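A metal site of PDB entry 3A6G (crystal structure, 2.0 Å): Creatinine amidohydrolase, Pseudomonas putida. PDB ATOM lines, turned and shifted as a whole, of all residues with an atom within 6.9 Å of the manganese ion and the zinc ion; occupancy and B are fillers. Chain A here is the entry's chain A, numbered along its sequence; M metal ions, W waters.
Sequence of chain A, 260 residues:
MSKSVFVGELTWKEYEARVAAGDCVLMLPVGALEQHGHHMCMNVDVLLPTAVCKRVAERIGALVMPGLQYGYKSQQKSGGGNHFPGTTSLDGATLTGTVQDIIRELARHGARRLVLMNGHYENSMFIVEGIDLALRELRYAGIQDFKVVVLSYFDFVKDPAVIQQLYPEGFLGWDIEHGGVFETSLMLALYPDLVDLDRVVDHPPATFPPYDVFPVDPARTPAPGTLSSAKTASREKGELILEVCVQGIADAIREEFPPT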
ATOM      1  N   GLY A  31     -28.838  11.518 -17.292  1.00  0.00           N
ATOM      2  CA  GLY A  31     -28.319  12.551 -16.425  1.00  0.00           C
ATOM      3  C   GLY A  31     -26.952  12.293 -15.816  1.00  0.00           C
ATOM      4  O   GLY A  31     -26.020  11.828 -16.477  1.00  0.00           O
ATOM      5  N   ALA A  32     -26.847  12.611 -14.527  1.00  0.00           N
ATOM      6  CA  ALA A  32     -25.597  12.448 -13.798  1.00  0.00           C
ATOM      7  C   ALA A  32     -25.795  12.768 -12.321  1.00  0.00           C
ATOM      8  O   ALA A  32     -26.809  13.328 -11.926  1.00  0.00           O
ATOM      9  CB  ALA A  32     -24.538  13.401 -14.374  1.00  0.00           C
ATOM     10  N   GLU A  34     -23.897  14.881  -9.842  1.00  0.00           N
ATOM     11  CA  GLU A  34     -22.849  15.893  -9.894  1.00  0.00           C
ATOM     12  C   GLU A  34     -23.126  17.066  -8.967  1.00  0.00           C
ATOM     13  O   GLU A  34     -24.265  17.492  -8.808  1.00  0.00           O
ATOM     14  CB  GLU A  34     -22.740  16.376 -11.344  1.00  0.00           C
ATOM     15  CG  GLU A  34     -21.753  17.518 -11.624  1.00  0.00           C
ATOM     16  CD  GLU A  34     -21.917  18.047 -13.038  1.00  0.00           C
ATOM     17  OE1 GLU A  34     -23.073  18.302 -13.427  1.00  0.00           O
ATOM     18  OE2 GLU A  34     -20.910  18.217 -13.764  1.00  0.00           O
ATOM     19  N   GLN A  35     -22.066  17.587  -8.369  1.00  0.00           N
ATOM     20  CA  GLN A  35     -22.184  18.713  -7.469  1.00  0.00           C
ATOM     21  C   GLN A  35     -22.847  19.869  -8.210  1.00  0.00           C
ATOM     22  O   GLN A  35     -22.599  20.084  -9.395  1.00  0.00           O
ATOM     23  CB  GLN A  35     -20.801  19.147  -6.964  1.00  0.00           C
ATOM     24  CG  GLN A  35     -19.871  19.770  -8.010  1.00  0.00           C
ATOM     25  CD  GLN A  35     -20.215  21.214  -8.341  1.00  0.00           C
ATOM     26  OE1 GLN A  35     -20.820  21.917  -7.538  1.00  0.00           O
ATOM     27  NE2 GLN A  35     -19.798  21.671  -9.528  1.00  0.00           N
ATOM     28  N   HIS A  36     -23.711  20.588  -7.505  1.00  0.00           N
ATOM     29  CA  HIS A  36     -24.402  21.739  -8.070  1.00  0.00           C
ATOM     30  C   HIS A  36     -24.383  22.902  -7.071  1.00  0.00           C
ATOM     31  O   HIS A  36     -25.430  23.467  -6.766  1.00  0.00           O
ATOM     32  CB  HIS A  36     -25.849  21.403  -8.428  1.00  0.00           C
ATOM     33  CG  HIS A  36     -25.996  20.773  -9.786  1.00  0.00           C
ATOM     34  ND1 HIS A  36     -25.649  19.475 -10.043  1.00  0.00           N
ATOM     35  CD2 HIS A  36     -26.426  21.296 -10.959  1.00  0.00           C
ATOM     36  CE1 HIS A  36     -25.858  19.210 -11.317  1.00  0.00           C
ATOM     37  NE2 HIS A  36     -26.328  20.300 -11.895  1.00  0.00           N
ATOM     38  N   MET A  40     -28.053  23.655  -4.061  1.00  0.00           N
ATOM     39  CA  MET A  40     -28.875  22.620  -4.689  1.00  0.00           C
ATOM     40  C   MET A  40     -28.308  21.208  -4.495  1.00  0.00           C
ATOM     41  O   MET A  40     -27.119  21.032  -4.257  1.00  0.00           O
ATOM     42  CB  MET A  40     -29.014  22.852  -6.194  1.00  0.00           C
ATOM     43  CG  MET A  40     -29.873  24.002  -6.605  1.00  0.00           C
ATOM     44  SD  MET A  40     -30.364  23.808  -8.329  1.00  0.00           S
ATOM     45  CE  MET A  40     -28.807  24.111  -9.182  1.00  0.00           C
ATOM     46  N   VAL A  44     -29.730  16.849  -9.741  1.00  0.00           N
ATOM     47  CA  VAL A  44     -30.370  17.795 -10.656  1.00  0.00           C
ATOM     48  C   VAL A  44     -30.378  17.358 -12.130  1.00  0.00           C
ATOM     49  O   VAL A  44     -31.408  17.445 -12.794  1.00  0.00           O
ATOM     50  CB  VAL A  44     -29.692  19.198 -10.573  1.00  0.00           C
ATOM     51  CG1 VAL A  44     -30.178  20.102 -11.708  1.00  0.00           C
ATOM     52  CG2 VAL A  44     -30.001  19.848  -9.215  1.00  0.00           C
ATOM     53  N   ASP A  45     -29.242  16.891 -12.627  1.00  0.00           N
ATOM     54  CA  ASP A  45     -29.141  16.469 -14.016  1.00  0.00           C
ATOM     55  C   ASP A  45     -30.000  15.280 -14.409  1.00  0.00           C
ATOM     56  O   ASP A  45     -30.184  15.015 -15.590  1.00  0.00           O
ATOM     57  CB  ASP A  45     -27.689  16.212 -14.393  1.00  0.00           C
ATOM     58  CG  ASP A  45     -26.920  17.500 -14.578  1.00  0.00           C
ATOM     59  OD1 ASP A  45     -27.540  18.570 -14.413  1.00  0.00           O
ATOM     60  OD2 ASP A  45     -25.713  17.441 -14.881  1.00  0.00           O
ATOM     61  N   LEU A  48     -34.230  16.993 -13.701  1.00  0.00           N
ATOM     62  CA  LEU A  48     -34.732  17.896 -14.729  1.00  0.00           C
ATOM     63  C   LEU A  48     -35.132  17.234 -16.052  1.00  0.00           C
ATOM     64  O   LEU A  48     -36.233  17.463 -16.541  1.00  0.00           O
ATOM     65  CB  LEU A  48     -33.743  19.043 -14.963  1.00  0.00           C
ATOM     66  CG  LEU A  48     -33.521  19.920 -13.721  1.00  0.00           C
ATOM     67  CD1 LEU A  48     -32.662  21.126 -14.084  1.00  0.00           C
ATOM     68  CD2 LEU A  48     -34.862  20.372 -13.152  1.00  0.00           C
ATOM     69  N   SER A  74     -17.477  15.025 -15.089  1.00  0.00           N
ATOM     70  CA  SER A  74     -17.722  16.458 -15.091  1.00  0.00           C
ATOM     71  C   SER A  74     -16.492  17.178 -15.612  1.00  0.00           C
ATOM     72  O   SER A  74     -15.360  16.861 -15.227  1.00  0.00           O
ATOM     73  CB  SER A  74     -18.031  16.930 -13.659  1.00  0.00           C
ATOM     74  OG  SER A  74     -18.233  18.343 -13.609  1.00  0.00           O
ATOM     75  N   SER A  78     -17.791  23.193 -17.837  1.00  0.00           N
ATOM     76  CA  SER A  78     -19.222  22.971 -17.946  1.00  0.00           C
ATOM     77  C   SER A  78     -19.881  22.436 -16.694  1.00  0.00           C
ATOM     78  O   SER A  78     -21.078  22.622 -16.481  1.00  0.00           O
ATOM     79  CB  SER A  78     -19.516  22.032 -19.126  1.00  0.00           C
ATOM     80  OG  SER A  78     -18.760  20.830 -19.011  1.00  0.00           O
ATOM     81  N   GLY A  79     -19.106  21.759 -15.840  1.00  0.00           N
ATOM     82  CA  GLY A  79     -19.672  21.215 -14.632  1.00  0.00           C
ATOM     83  C   GLY A  79     -18.855  21.459 -13.381  1.00  0.00           C
ATOM     84  O   GLY A  79     -19.219  20.983 -12.306  1.00  0.00           O
ATOM     85  N   GLY A 119     -29.419  15.641 -19.902  1.00  0.00           N
ATOM     86  CA  GLY A 119     -29.480  16.712 -18.925  1.00  0.00           C
ATOM     87  C   GLY A 119     -28.104  17.109 -18.406  1.00  0.00           C
ATOM     88  O   GLY A 119     -27.990  18.040 -17.609  1.00  0.00           O
ATOM     89  N   HIS A 120     -27.069  16.419 -18.875  1.00  0.00           N
ATOM     90  CA  HIS A 120     -25.685  16.666 -18.465  1.00  0.00           C
ATOM     91  C   HIS A 120     -24.849  16.854 -19.731  1.00  0.00           C
ATOM     92  O   HIS A 120     -24.580  15.898 -20.459  1.00  0.00           O
ATOM     93  CB  HIS A 120     -25.191  15.443 -17.659  1.00  0.00           C
ATOM     94  CG  HIS A 120     -23.776  15.538 -17.178  1.00  0.00           C
ATOM     95  ND1 HIS A 120     -23.316  16.550 -16.365  1.00  0.00           N
ATOM     96  CD2 HIS A 120     -22.725  14.680 -17.343  1.00  0.00           C
ATOM     97  CE1 HIS A 120     -22.053  16.320 -16.037  1.00  0.00           C
ATOM     98  NE2 HIS A 120     -21.672  15.196 -16.619  1.00  0.00           N
ATOM     99  N   TYR A 121     -24.444  18.096 -19.990  1.00  0.00           N
ATOM    100  CA  TYR A 121     -23.685  18.463 -21.185  1.00  0.00           C
ATOM    101  C   TYR A 121     -22.595  17.476 -21.618  1.00  0.00           C
ATOM    102  O   TYR A 121     -22.516  17.098 -22.787  1.00  0.00           O
ATOM    103  CB  TYR A 121     -23.069  19.857 -21.012  1.00  0.00           C
ATOM    104  CG  TYR A 121     -22.358  20.370 -22.242  1.00  0.00           C
ATOM    105  CD1 TYR A 121     -23.066  20.646 -23.414  1.00  0.00           C
ATOM    106  CD2 TYR A 121     -20.979  20.557 -22.249  1.00  0.00           C
ATOM    107  CE1 TYR A 121     -22.418  21.101 -24.565  1.00  0.00           C
ATOM    108  CE2 TYR A 121     -20.325  21.015 -23.391  1.00  0.00           C
ATOM    109  CZ  TYR A 121     -21.046  21.290 -24.543  1.00  0.00           C
ATOM    110  OH  TYR A 121     -20.397  21.744 -25.670  1.00  0.00           O
ATOM    111  N   GLU A 122     -21.760  17.077 -20.661  1.00  0.00           N
ATOM    112  CA  GLU A 122     -20.654  16.160 -20.930  1.00  0.00           C
ATOM    113  C   GLU A 122     -21.033  14.785 -21.499  1.00  0.00           C
ATOM    114  O   GLU A 122     -20.177  14.099 -22.063  1.00  0.00           O
ATOM    115  CB  GLU A 122     -19.832  15.973 -19.647  1.00  0.00           C
ATOM    116  CG  GLU A 122     -19.107  17.243 -19.181  1.00  0.00           C
ATOM    117  CD  GLU A 122     -19.943  18.116 -18.257  1.00  0.00           C
ATOM    118  OE1 GLU A 122     -21.182  18.202 -18.438  1.00  0.00           O
ATOM    119  OE2 GLU A 122     -19.361  18.742 -17.353  1.00  0.00           O
ATOM    120  N   TYR A 153     -32.541  19.160 -23.300  1.00  0.00           N
ATOM    121  CA  TYR A 153     -33.690  20.011 -23.022  1.00  0.00           C
ATOM    122  C   TYR A 153     -33.339  21.491 -22.961  1.00  0.00           C
ATOM    123  O   TYR A 153     -34.167  22.336 -23.308  1.00  0.00           O
ATOM    124  CB  TYR A 153     -34.361  19.555 -21.711  1.00  0.00           C
ATOM    125  CG  TYR A 153     -33.638  19.989 -20.455  1.00  0.00           C
ATOM    126  CD1 TYR A 153     -33.709  21.309 -20.025  1.00  0.00           C
ATOM    127  CD2 TYR A 153     -32.864  19.084 -19.718  1.00  0.00           C
ATOM    128  CE1 TYR A 153     -33.033  21.726 -18.891  1.00  0.00           C
ATOM    129  CE2 TYR A 153     -32.175  19.501 -18.581  1.00  0.00           C
ATOM    130  CZ  TYR A 153     -32.268  20.825 -18.175  1.00  0.00           C
ATOM    131  OH  TYR A 153     -31.601  21.271 -17.056  1.00  0.00           O
ATOM    132  N   GLU A 177     -23.935  28.133 -17.469  1.00  0.00           N
ATOM    133  CA  GLU A 177     -25.136  27.804 -16.735  1.00  0.00           C
ATOM    134  C   GLU A 177     -25.112  26.531 -15.888  1.00  0.00           C
ATOM    135  O   GLU A 177     -26.082  25.770 -15.881  1.00  0.00           O
ATOM    136  CB  GLU A 177     -26.333  27.738 -17.701  1.00  0.00           C
ATOM    137  CG  GLU A 177     -26.978  29.081 -17.996  1.00  0.00           C
ATOM    138  CD  GLU A 177     -27.507  29.760 -16.738  1.00  0.00           C
ATOM    139  OE1 GLU A 177     -28.132  29.074 -15.902  1.00  0.00           O
ATOM    140  OE2 GLU A 177     -27.320  30.987 -16.590  1.00  0.00           O
ATOM    141  N   HIS A 178     -24.006  26.272 -15.187  1.00  0.00           N
ATOM    142  CA  HIS A 178     -23.963  25.105 -14.309  1.00  0.00           C
ATOM    143  C   HIS A 178     -24.277  25.610 -12.907  1.00  0.00           C
ATOM    144  O   HIS A 178     -23.499  26.372 -12.333  1.00  0.00           O
ATOM    145  CB  HIS A 178     -22.588  24.442 -14.307  1.00  0.00           C
ATOM    146  CG  HIS A 178     -22.469  23.348 -13.290  1.00  0.00           C
ATOM    147  ND1 HIS A 178     -23.198  22.175 -13.357  1.00  0.00           N
ATOM    148  CD2 HIS A 178     -21.743  23.264 -12.146  1.00  0.00           C
ATOM    149  CE1 HIS A 178     -22.932  21.430 -12.298  1.00  0.00           C
ATOM    150  NE2 HIS A 178     -22.048  22.068 -11.550  1.00  0.00           N
ATOM    151  N   GLY A 179     -25.420  25.207 -12.370  1.00  0.00           N
ATOM    152  CA  GLY A 179     -25.823  25.625 -11.034  1.00  0.00           C
ATOM    153  C   GLY A 179     -26.215  27.092 -10.977  1.00  0.00           C
ATOM    154  O   GLY A 179     -26.278  27.682  -9.901  1.00  0.00           O
ATOM    155  N   GLU A 183     -30.896  26.274 -14.243  1.00  0.00           N
ATOM    156  CA  GLU A 183     -31.206  25.057 -13.505  1.00  0.00           C
ATOM    157  C   GLU A 183     -31.869  25.312 -12.167  1.00  0.00           C
ATOM    158  O   GLU A 183     -32.791  24.605 -11.769  1.00  0.00           O
ATOM    159  CB  GLU A 183     -29.933  24.237 -13.275  1.00  0.00           C
ATOM    160  CG  GLU A 183     -29.227  23.821 -14.535  1.00  0.00           C
ATOM    161  CD  GLU A 183     -28.087  22.881 -14.249  1.00  0.00           C
ATOM    162  OE1 GLU A 183     -28.204  21.705 -14.637  1.00  0.00           O
ATOM    163  OE2 GLU A 183     -27.096  23.313 -13.631  1.00  0.00           O
HETATM  164 MN    MN M   1     -23.996  18.457 -15.353  1.00  0.00          MN
HETATM  165 ZN    ZN M   2     -26.658  20.423 -14.025  1.00  0.00          ZN
HETATM  166  O   HOH W   1     -22.113  19.529 -16.066  1.00  0.00           O
HETATM  167  O   HOH W   2     -24.768  20.602 -15.040  1.00  0.00           O
HETATM  168  O   HOH W   3     -25.357  20.218 -17.450  1.00  0.00           O
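The backbone NH (N) of Gly 179 sits at hydrogen-bond distance from the side-chain carboxylate (OE2) of Glu 183 (2.8 Å). ND1 of His 36 lies within hydrogen-bond range of O of Glu 34. OG of Ser 74 sits at hydrogen-bond distance from OE2 of Glu 34. A ring nitrogen (ND1) of His 120 lies close to the side-chain carboxylate of Glu 122, 3.4 Å away. NE2 of His 178 sits at hydrogen-bond distance from O of Gly 79 (3.1 Å). A ring nitrogen (NE2) of His 178 lies within hydrogen-bond range of the backbone carbonyl oxygen of Gln 35 (3.0 Å).
Three residues have an atom within 4 Å of the manganese ion: Glu 34, Asp 45 and His 120. The nearest printed residue that does not touch the manganese ion is Glu 122 (4.2 Å).
Merely in contact with the zinc ion: His 178 (3.9 Å). Within 4 Å of the zinc ion: His 36, Asp 45, His 178 and Glu 183. The nearest printed residue that does not touch the zinc ion is Glu 34 (4.2 Å).
The manganese ion is bound by OD2 of Asp 45 (2.1 Å), OE1 of Glu 34 (2.1 Å), ND1 of His 120 (2.3 Å), water W1 (2.3 Å) and water W2 (2.3 Å).
The zinc ion is bound by OD1 of Asp 45 (2.1 Å), OE1 of Glu 183 (2.1 Å), water W2 (2.2 Å) and NE2 of His 36 (2.2 Å).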
